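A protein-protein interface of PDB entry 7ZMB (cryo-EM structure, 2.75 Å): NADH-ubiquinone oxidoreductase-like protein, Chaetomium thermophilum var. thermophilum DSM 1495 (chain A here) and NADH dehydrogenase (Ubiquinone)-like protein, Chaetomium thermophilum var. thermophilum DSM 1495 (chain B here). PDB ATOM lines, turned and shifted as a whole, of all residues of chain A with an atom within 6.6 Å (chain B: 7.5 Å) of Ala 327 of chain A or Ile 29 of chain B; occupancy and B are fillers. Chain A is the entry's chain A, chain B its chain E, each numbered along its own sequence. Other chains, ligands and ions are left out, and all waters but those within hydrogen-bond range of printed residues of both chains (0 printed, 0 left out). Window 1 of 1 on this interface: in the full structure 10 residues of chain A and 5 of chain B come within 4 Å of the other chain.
Printed residues of chain B within 4 Å of Met 315 of chain A: Pro 37 (3.5 Å) and Ile 39 (3.6 Å). Of the printed residues of chain B, Pro 316 of chain A touches Ile 29. Of chain B, only Ile 29 (3.8 Å) and Ile 31 (3.8 Å) come within 4 Å of Ala 327 of chain A. Of the printed residues of chain B, Gln 331 of chain A touches Ile 31. Of the printed residues of chain B, Ala 624 of chain A touches Asp 28, Ile 29 and Ile 39. Ile 29 of chain B touches just these residues of chain A: Pro 316 (3.6 Å), Ala 327 (3.8 Å), Thr 328 (3.5 Å), Trp 329 (3.9 Å) and Ala 624 (3.6 Å). Of the printed residues of chain A, Pro 37 of chain B touches Met 315 and Pro 326. The nearest printed residue of chain B that does not touch Trp 329 of chain A is Asp 28 of chain B (4.2 Å).
CE of Met 315 of chain A touches CB of Pro 37 of chain B, at 3.5 Å. Met 315 of chain A touches Ile 39 of chain B. Ile 29 of chain B touches Pro 316 of chain A. Pro 326 of chain A touches Ile 31 of chain B (O to CD1, 3.3 Å). Pro 37 of chain B touches Pro 326 of chain A (CG to CG, 3.7 Å). Ile 29 of chain B touches Ala 327 of chain A. Ala 327 of chain A touches Ile 31 of chain B (CA to CD1, 3.8 Å). Trp 329 of chain A touches Ile 29 of chain B (CD1 to CD1, 3.9 Å). Ile 31 of chain B touches Gln 331 of chain A (CD1 to OE1, 3.6 Å). CD1 of Ile 29 of chain B touches CB of Ala 624 of chain A (3.6 Å).
The side-chain hydroxyl of Ser 27 of chain B is in hydrogen-bond range of the side-chain carboxylate of Asp 28 of chain B, 3.3 Å away. The side-chain hydroxyl (OG) of Ser 27 of chain B lies within hydrogen-bond range of the backbone NH (N) of Ile 29 of chain B (3.1 Å). The backbone carbonyl oxygen of Pro 316 of chain A is in hydrogen-bond range of the backbone NH of Ala 327 of chain A (2.7 Å). The side-chain amide oxygen (OE1) of Gln 331 of chain A sits at hydrogen-bond distance from the backbone NH (N) of Thr 328 of chain A, 3.0 Å away. The indole nitrogen (NE1) of Trp 329 of chain A is in hydrogen-bond range of the backbone carbonyl oxygen (O) of Ala 624 of chain A. The guanidinium group of Arg 626 of chain A lies within hydrogen-bond range of the backbone carbonyl oxygen of Ala 624 of chain A (3.1 Å).
OD1 of Asp 28 of chain B lies within salt-bridge range of NH2 of Arg 626 of chain A (2.7 Å). O of Ile 29 of chain B lies within hydrogen-bond range of OG1 of Thr 328 of chain A (3.5 Å).
Printed residues of chain A that touch a printed residue of chain B: Met 315, Pro 316, Pro 326, Ala 327, Thr 328, Trp 329, Gln 331, Ala 624 and Arg 626. Of the 12 printed residues of chain B, 5 touch a printed residue of chain A.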
ATOM      1  N   THR A 314     -17.094  23.333  -0.018  1.00  0.00           N
ATOM      2  CA  THR A 314     -16.177  23.907  -0.985  1.00  0.00           C
ATOM      3  C   THR A 314     -16.145  23.167  -2.308  1.00  0.00           C
ATOM      4  O   THR A 314     -15.532  23.666  -3.252  1.00  0.00           O
ATOM      5  CB  THR A 314     -14.751  23.961  -0.419  1.00  0.00           C
ATOM      6  OG1 THR A 314     -14.394  22.678   0.105  1.00  0.00           O
ATOM      7  CG2 THR A 314     -14.647  25.004   0.677  1.00  0.00           C
ATOM      8  N   MET A 315     -16.774  22.005  -2.410  1.00  0.00           N
ATOM      9  CA  MET A 315     -16.709  21.214  -3.622  1.00  0.00           C
ATOM     10  C   MET A 315     -18.051  20.554  -3.873  1.00  0.00           C
ATOM     11  O   MET A 315     -18.790  20.260  -2.927  1.00  0.00           O
ATOM     12  CB  MET A 315     -15.618  20.148  -3.503  1.00  0.00           C
ATOM     13  CG  MET A 315     -15.644  19.442  -2.163  1.00  0.00           C
ATOM     14  SD  MET A 315     -14.587  18.010  -2.187  1.00  0.00           S
ATOM     15  CE  MET A 315     -13.197  18.762  -2.991  1.00  0.00           C
ATOM     16  N   PRO A 316     -18.403  20.326  -5.135  1.00  0.00           N
ATOM     17  CA  PRO A 316     -19.612  19.551  -5.425  1.00  0.00           C
ATOM     18  C   PRO A 316     -19.441  18.100  -5.010  1.00  0.00           C
ATOM     19  O   PRO A 316     -18.408  17.479  -5.262  1.00  0.00           O
ATOM     20  CB  PRO A 316     -19.764  19.691  -6.941  1.00  0.00           C
ATOM     21  CG  PRO A 316     -19.010  20.911  -7.285  1.00  0.00           C
ATOM     22  CD  PRO A 316     -17.861  20.968  -6.340  1.00  0.00           C
ATOM     23  N   LEU A 317     -20.466  17.559  -4.361  1.00  0.00           N
ATOM     24  CA  LEU A 317     -20.474  16.170  -3.938  1.00  0.00           C
ATOM     25  C   LEU A 317     -21.662  15.462  -4.565  1.00  0.00           C
ATOM     26  O   LEU A 317     -22.794  15.940  -4.475  1.00  0.00           O
ATOM     27  CB  LEU A 317     -20.540  16.043  -2.417  1.00  0.00           C
ATOM     28  CG  LEU A 317     -19.464  16.780  -1.632  1.00  0.00           C
ATOM     29  CD1 LEU A 317     -19.814  16.766  -0.168  1.00  0.00           C
ATOM     30  CD2 LEU A 317     -18.096  16.170  -1.879  1.00  0.00           C
ATOM     31  N   VAL A 318     -21.399  14.323  -5.193  1.00  0.00           N
ATOM     32  CA  VAL A 318     -22.432  13.465  -5.747  1.00  0.00           C
ATOM     33  C   VAL A 318     -22.514  12.220  -4.882  1.00  0.00           C
ATOM     34  O   VAL A 318     -21.493  11.584  -4.603  1.00  0.00           O
ATOM     35  CB  VAL A 318     -22.142  13.101  -7.214  1.00  0.00           C
ATOM     36  CG1 VAL A 318     -23.206  12.171  -7.750  1.00  0.00           C
ATOM     37  CG2 VAL A 318     -22.064  14.343  -8.048  1.00  0.00           C
ATOM     38  N   ARG A 320     -22.762   8.620  -4.251  1.00  0.00           N
ATOM     39  CA  ARG A 320     -22.508   7.400  -4.999  1.00  0.00           C
ATOM     40  C   ARG A 320     -22.381   6.257  -4.013  1.00  0.00           C
ATOM     41  O   ARG A 320     -21.504   6.282  -3.146  1.00  0.00           O
ATOM     42  CB  ARG A 320     -21.250   7.524  -5.862  1.00  0.00           C
ATOM     43  CG  ARG A 320     -21.372   8.576  -6.949  1.00  0.00           C
ATOM     44  CD  ARG A 320     -20.493   8.271  -8.139  1.00  0.00           C
ATOM     45  NE  ARG A 320     -20.718   9.232  -9.214  1.00  0.00           N
ATOM     46  CZ  ARG A 320     -19.925  10.265  -9.472  1.00  0.00           C
ATOM     47  NH1 ARG A 320     -20.213  11.088 -10.469  1.00  0.00           N
ATOM     48  NH2 ARG A 320     -18.844  10.476  -8.735  1.00  0.00           N
ATOM     49  N   GLU A 325     -18.962  11.623  -2.793  1.00  0.00           N
ATOM     50  CA  GLU A 325     -17.670  11.763  -3.443  1.00  0.00           C
ATOM     51  C   GLU A 325     -17.543  13.106  -4.148  1.00  0.00           C
ATOM     52  O   GLU A 325     -18.533  13.664  -4.624  1.00  0.00           O
ATOM     53  CB  GLU A 325     -17.428  10.632  -4.446  1.00  0.00           C
ATOM     54  CG  GLU A 325     -17.265   9.275  -3.794  1.00  0.00           C
ATOM     55  CD  GLU A 325     -18.582   8.625  -3.460  1.00  0.00           C
ATOM     56  OE1 GLU A 325     -19.632   9.209  -3.791  1.00  0.00           O
ATOM     57  OE2 GLU A 325     -18.567   7.523  -2.883  1.00  0.00           O
ATOM     58  N   PRO A 326     -16.332  13.656  -4.206  1.00  0.00           N
ATOM     59  CA  PRO A 326     -16.130  14.923  -4.908  1.00  0.00           C
ATOM     60  C   PRO A 326     -16.497  14.821  -6.377  1.00  0.00           C
ATOM     61  O   PRO A 326     -16.336  13.782  -7.017  1.00  0.00           O
ATOM     62  CB  PRO A 326     -14.632  15.201  -4.734  1.00  0.00           C
ATOM     63  CG  PRO A 326     -14.159  14.313  -3.690  1.00  0.00           C
ATOM     64  CD  PRO A 326     -15.206  13.317  -3.326  1.00  0.00           C
ATOM     65  N   ALA A 327     -17.002  15.925  -6.906  1.00  0.00           N
ATOM     66  CA  ALA A 327     -17.306  16.039  -8.317  1.00  0.00           C
ATOM     67  C   ALA A 327     -16.813  17.378  -8.839  1.00  0.00           C
ATOM     68  O   ALA A 327     -16.789  18.380  -8.124  1.00  0.00           O
ATOM     69  CB  ALA A 327     -18.806  15.895  -8.587  1.00  0.00           C
ATOM     70  N   THR A 328     -16.398  17.365 -10.097  1.00  0.00           N
ATOM     71  CA  THR A 328     -16.215  18.581 -10.866  1.00  0.00           C
ATOM     72  C   THR A 328     -17.564  19.264 -11.060  1.00  0.00           C
ATOM     73  O   THR A 328     -18.611  18.615 -11.058  1.00  0.00           O
ATOM     74  CB  THR A 328     -15.566  18.221 -12.210  1.00  0.00           C
ATOM     75  OG1 THR A 328     -14.201  17.859 -11.985  1.00  0.00           O
ATOM     76  CG2 THR A 328     -15.628  19.359 -13.211  1.00  0.00           C
ATOM     77  N   TRP A 329     -17.543  20.591 -11.206  1.00  0.00           N
ATOM     78  CA  TRP A 329     -18.781  21.330 -11.436  1.00  0.00           C
ATOM     79  C   TRP A 329     -19.511  20.828 -12.674  1.00  0.00           C
ATOM     80  O   TRP A 329     -20.741  20.734 -12.679  1.00  0.00           O
ATOM     81  CB  TRP A 329     -18.494  22.823 -11.558  1.00  0.00           C
ATOM     82  CG  TRP A 329     -18.582  23.556 -10.266  1.00  0.00           C
ATOM     83  CD1 TRP A 329     -17.545  24.044  -9.539  1.00  0.00           C
ATOM     84  CD2 TRP A 329     -19.769  23.873  -9.537  1.00  0.00           C
ATOM     85  NE1 TRP A 329     -18.006  24.651  -8.406  1.00  0.00           N
ATOM     86  CE2 TRP A 329     -19.370  24.561  -8.377  1.00  0.00           C
ATOM     87  CE3 TRP A 329     -21.128  23.641  -9.748  1.00  0.00           C
ATOM     88  CZ2 TRP A 329     -20.280  25.020  -7.432  1.00  0.00           C
ATOM     89  CZ3 TRP A 329     -22.029  24.106  -8.815  1.00  0.00           C
ATOM     90  CH2 TRP A 329     -21.603  24.786  -7.672  1.00  0.00           C
ATOM     91  N   GLU A 330     -18.772  20.497 -13.734  1.00  0.00           N
ATOM     92  CA  GLU A 330     -19.402  19.951 -14.930  1.00  0.00           C
ATOM     93  C   GLU A 330     -20.041  18.597 -14.658  1.00  0.00           C
ATOM     94  O   GLU A 330     -21.167  18.338 -15.091  1.00  0.00           O
ATOM     95  CB  GLU A 330     -18.382  19.836 -16.057  1.00  0.00           C
ATOM     96  CG  GLU A 330     -18.995  19.658 -17.429  1.00  0.00           C
ATOM     97  CD  GLU A 330     -18.225  20.396 -18.501  1.00  0.00           C
ATOM     98  OE1 GLU A 330     -18.544  20.221 -19.697  1.00  0.00           O
ATOM     99  OE2 GLU A 330     -17.285  21.140 -18.150  1.00  0.00           O
ATOM    100  N   GLN A 331     -19.352  17.720 -13.938  1.00  0.00           N
ATOM    101  CA  GLN A 331     -19.889  16.385 -13.739  1.00  0.00           C
ATOM    102  C   GLN A 331     -20.903  16.337 -12.612  1.00  0.00           C
ATOM    103  O   GLN A 331     -21.441  15.266 -12.324  1.00  0.00           O
ATOM    104  CB  GLN A 331     -18.761  15.378 -13.493  1.00  0.00           C
ATOM    105  CG  GLN A 331     -17.971  15.575 -12.229  1.00  0.00           C
ATOM    106  CD  GLN A 331     -16.843  14.577 -12.104  1.00  0.00           C
ATOM    107  OE1 GLN A 331     -16.065  14.624 -11.154  1.00  0.00           O
ATOM    108  NE2 GLN A 331     -16.732  13.683 -13.070  1.00  0.00           N
ATOM    109  N   ALA A 332     -21.174  17.471 -11.975  1.00  0.00           N
ATOM    110  CA  ALA A 332     -22.271  17.620 -11.032  1.00  0.00           C
ATOM    111  C   ALA A 332     -23.510  18.215 -11.679  1.00  0.00           C
ATOM    112  O   ALA A 332     -24.621  17.754 -11.413  1.00  0.00           O
ATOM    113  CB  ALA A 332     -21.838  18.495  -9.853  1.00  0.00           C
ATOM    114  N   ALA A 624     -13.990  25.901  -4.123  1.00  0.00           N
ATOM    115  CA  ALA A 624     -14.612  25.897  -5.438  1.00  0.00           C
ATOM    116  C   ALA A 624     -16.078  26.299  -5.369  1.00  0.00           C
ATOM    117  O   ALA A 624     -16.873  25.910  -6.223  1.00  0.00           O
ATOM    118  CB  ALA A 624     -14.458  24.531  -6.095  1.00  0.00           C
ATOM    119  N   ARG A 626     -19.374  28.733  -5.645  1.00  0.00           N
ATOM    120  CA  ARG A 626     -19.823  29.696  -6.630  1.00  0.00           C
ATOM    121  C   ARG A 626     -20.826  30.635  -5.989  1.00  0.00           C
ATOM    122  O   ARG A 626     -21.275  30.428  -4.863  1.00  0.00           O
ATOM    123  CB  ARG A 626     -20.452  29.004  -7.843  1.00  0.00           C
ATOM    124  CG  ARG A 626     -19.507  28.142  -8.611  1.00  0.00           C
ATOM    125  CD  ARG A 626     -18.453  28.947  -9.308  1.00  0.00           C
ATOM    126  NE  ARG A 626     -17.763  28.142 -10.305  1.00  0.00           N
ATOM    127  CZ  ARG A 626     -16.671  27.429 -10.061  1.00  0.00           C
ATOM    128  NH1 ARG A 626     -16.133  27.424  -8.847  1.00  0.00           N
ATOM    129  NH2 ARG A 626     -16.117  26.729 -11.034  1.00  0.00           N
ATOM    130  N   ILE B  26      -8.056  22.253 -16.699  1.00  0.00           N
ATOM    131  CA  ILE B  26      -8.948  23.082 -17.497  1.00  0.00           C
ATOM    132  C   ILE B  26      -9.984  23.732 -16.599  1.00  0.00           C
ATOM    133  O   ILE B  26     -10.429  24.844 -16.850  1.00  0.00           O
ATOM    134  CB  ILE B  26      -9.628  22.272 -18.607  1.00  0.00           C
ATOM    135  CG1 ILE B  26     -10.155  20.946 -18.055  1.00  0.00           C
ATOM    136  CG2 ILE B  26      -8.659  22.027 -19.750  1.00  0.00           C
ATOM    137  CD1 ILE B  26     -11.133  20.251 -18.973  1.00  0.00           C
ATOM    138  N   SER B  27     -10.356  23.027 -15.547  1.00  0.00           N
ATOM    139  CA  SER B  27     -11.335  23.494 -14.587  1.00  0.00           C
ATOM    140  C   SER B  27     -10.624  24.003 -13.344  1.00  0.00           C
ATOM    141  O   SER B  27      -9.395  24.052 -13.273  1.00  0.00           O
ATOM    142  CB  SER B  27     -12.319  22.376 -14.239  1.00  0.00           C
ATOM    143  OG  SER B  27     -13.115  22.727 -13.124  1.00  0.00           O
ATOM    144  N   ASP B  28     -11.412  24.391 -12.356  1.00  0.00           N
ATOM    145  CA  ASP B  28     -10.864  24.713 -11.053  1.00  0.00           C
ATOM    146  C   ASP B  28     -10.812  23.503 -10.132  1.00  0.00           C
ATOM    147  O   ASP B  28     -10.238  23.598  -9.047  1.00  0.00           O
ATOM    148  CB  ASP B  28     -11.670  25.848 -10.403  1.00  0.00           C
ATOM    149  CG  ASP B  28     -13.121  25.486 -10.171  1.00  0.00           C
ATOM    150  OD1 ASP B  28     -13.848  25.250 -11.150  1.00  0.00           O
ATOM    151  OD2 ASP B  28     -13.538  25.447  -9.004  1.00  0.00           O
ATOM    152  N   ILE B  29     -11.387  22.375 -10.538  1.00  0.00           N
ATOM    153  CA  ILE B  29     -11.333  21.135  -9.770  1.00  0.00           C
ATOM    154  C   ILE B  29     -10.769  20.035 -10.657  1.00  0.00           C
ATOM    155  O   ILE B  29     -11.321  19.742 -11.722  1.00  0.00           O
ATOM    156  CB  ILE B  29     -12.709  20.728  -9.226  1.00  0.00           C
ATOM    157  CG1 ILE B  29     -13.476  21.944  -8.728  1.00  0.00           C
ATOM    158  CG2 ILE B  29     -12.551  19.730  -8.104  1.00  0.00           C
ATOM    159  CD1 ILE B  29     -14.854  21.612  -8.216  1.00  0.00           C
ATOM    160  N   HIS B  30      -9.683  19.419 -10.212  1.00  0.00           N
ATOM    161  CA  HIS B  30      -9.157  18.205 -10.814  1.00  0.00           C
ATOM    162  C   HIS B  30      -9.309  17.074  -9.811  1.00  0.00           C
ATOM    163  O   HIS B  30      -9.000  17.243  -8.632  1.00  0.00           O
ATOM    164  CB  HIS B  30      -7.685  18.356 -11.211  1.00  0.00           C
ATOM    165  CG  HIS B  30      -7.447  19.301 -12.346  1.00  0.00           C
ATOM    166  ND1 HIS B  30      -6.186  19.583 -12.821  1.00  0.00           N
ATOM    167  CD2 HIS B  30      -8.304  20.039 -13.091  1.00  0.00           C
ATOM    168  CE1 HIS B  30      -6.278  20.450 -13.814  1.00  0.00           C
ATOM    169  NE2 HIS B  30      -7.553  20.744 -13.996  1.00  0.00           N
ATOM    170  N   ILE B  31      -9.787  15.932 -10.280  1.00  0.00           N
ATOM    171  CA  ILE B  31      -9.922  14.736  -9.462  1.00  0.00           C
ATOM    172  C   ILE B  31      -9.032  13.661 -10.066  1.00  0.00           C
ATOM    173  O   ILE B  31      -9.084  13.415 -11.275  1.00  0.00           O
ATOM    174  CB  ILE B  31     -11.389  14.278  -9.372  1.00  0.00           C
ATOM    175  CG1 ILE B  31     -12.252  15.416  -8.831  1.00  0.00           C
ATOM    176  CG2 ILE B  31     -11.512  13.046  -8.499  1.00  0.00           C
ATOM    177  CD1 ILE B  31     -13.660  15.033  -8.525  1.00  0.00           C
ATOM    178  N   LYS B  36      -8.306  11.744  -5.018  1.00  0.00           N
ATOM    179  CA  LYS B  36      -8.126  12.981  -4.288  1.00  0.00           C
ATOM    180  C   LYS B  36      -8.552  14.159  -5.158  1.00  0.00           C
ATOM    181  O   LYS B  36      -8.318  14.157  -6.370  1.00  0.00           O
ATOM    182  CB  LYS B  36      -6.675  13.149  -3.837  1.00  0.00           C
ATOM    183  CG  LYS B  36      -5.643  13.007  -4.937  1.00  0.00           C
ATOM    184  CD  LYS B  36      -4.240  12.931  -4.364  1.00  0.00           C
ATOM    185  CE  LYS B  36      -4.024  11.636  -3.600  1.00  0.00           C
ATOM    186  NZ  LYS B  36      -2.603  11.462  -3.197  1.00  0.00           N
ATOM    187  N   PRO B  37      -9.211  15.156  -4.582  1.00  0.00           N
ATOM    188  CA  PRO B  37      -9.550  16.362  -5.331  1.00  0.00           C
ATOM    189  C   PRO B  37      -8.458  17.410  -5.227  1.00  0.00           C
ATOM    190  O   PRO B  37      -7.672  17.448  -4.279  1.00  0.00           O
ATOM    191  CB  PRO B  37     -10.840  16.838  -4.653  1.00  0.00           C
ATOM    192  CG  PRO B  37     -10.900  16.135  -3.348  1.00  0.00           C
ATOM    193  CD  PRO B  37      -9.766  15.180  -3.226  1.00  0.00           C
ATOM    194  N   LEU B  38      -8.415  18.271  -6.234  1.00  0.00           N
ATOM    195  CA  LEU B  38      -7.434  19.350  -6.294  1.00  0.00           C
ATOM    196  C   LEU B  38      -8.181  20.634  -6.625  1.00  0.00           C
ATOM    197  O   LEU B  38      -8.610  20.835  -7.764  1.00  0.00           O
ATOM    198  CB  LEU B  38      -6.345  19.048  -7.317  1.00  0.00           C
ATOM    199  CG  LEU B  38      -5.495  17.813  -7.002  1.00  0.00           C
ATOM    200  CD1 LEU B  38      -4.655  17.403  -8.203  1.00  0.00           C
ATOM    201  CD2 LEU B  38      -4.629  18.045  -5.788  1.00  0.00           C
ATOM    202  N   ILE B  39      -8.347  21.492  -5.627  1.00  0.00           N
ATOM    203  CA  ILE B  39      -9.024  22.770  -5.806  1.00  0.00           C
ATOM    204  C   ILE B  39      -7.968  23.791  -6.197  1.00  0.00           C
ATOM    205  O   ILE B  39      -7.131  24.175  -5.378  1.00  0.00           O
ATOM    206  CB  ILE B  39      -9.766  23.198  -4.537  1.00  0.00           C
ATOM    207  CG1 ILE B  39     -10.480  22.007  -3.897  1.00  0.00           C
ATOM    208  CG2 ILE B  39     -10.740  24.291  -4.855  1.00  0.00           C
ATOM    209  CD1 ILE B  39     -11.657  21.520  -4.656  1.00  0.00           C
ATOM    210  N   ARG B  40      -8.026  24.257  -7.437  1.00  0.00           N
ATOM    211  CA  ARG B  40      -6.950  25.033  -8.026  1.00  0.00           C
ATOM    212  C   ARG B  40      -7.282  26.517  -8.126  1.00  0.00           C
ATOM    213  O   ARG B  40      -8.434  26.911  -8.305  1.00  0.00           O
ATOM    214  CB  ARG B  40      -6.615  24.490  -9.410  1.00  0.00           C
ATOM    215  CG  ARG B  40      -5.963  23.132  -9.366  1.00  0.00           C
ATOM    216  CD  ARG B  40      -6.354  22.294 -10.557  1.00  0.00           C
ATOM    217  NE  ARG B  40      -6.396  23.058 -11.802  1.00  0.00           N
ATOM    218  CZ  ARG B  40      -5.326  23.405 -12.508  1.00  0.00           C
ATOM    219  NH1 ARG B  40      -5.473  24.080 -13.635  1.00  0.00           N
ATOM    220  NH2 ARG B  40      -4.112  23.085 -12.089  1.00  0.00           N
ATOM    221  N   GLN B  42      -5.707  29.465 -10.644  1.00  0.00           N
ATOM    222  CA  GLN B  42      -5.113  29.126 -11.932  1.00  0.00           C
ATOM    223  C   GLN B  42      -3.796  29.852 -12.197  1.00  0.00           C
ATOM    224  O   GLN B  42      -2.742  29.217 -12.317  1.00  0.00           O
ATOM    225  CB  GLN B  42      -6.112  29.404 -13.048  1.00  0.00           C
ATOM    226  CG  GLN B  42      -7.475  28.787 -12.806  1.00  0.00           C
ATOM    227  CD  GLN B  42      -7.497  27.284 -13.020  1.00  0.00           C
ATOM    228  OE1 GLN B  42      -6.543  26.582 -12.692  1.00  0.00           O
ATOM    229  NE2 GLN B  42      -8.591  26.785 -13.583  1.00  0.00           N
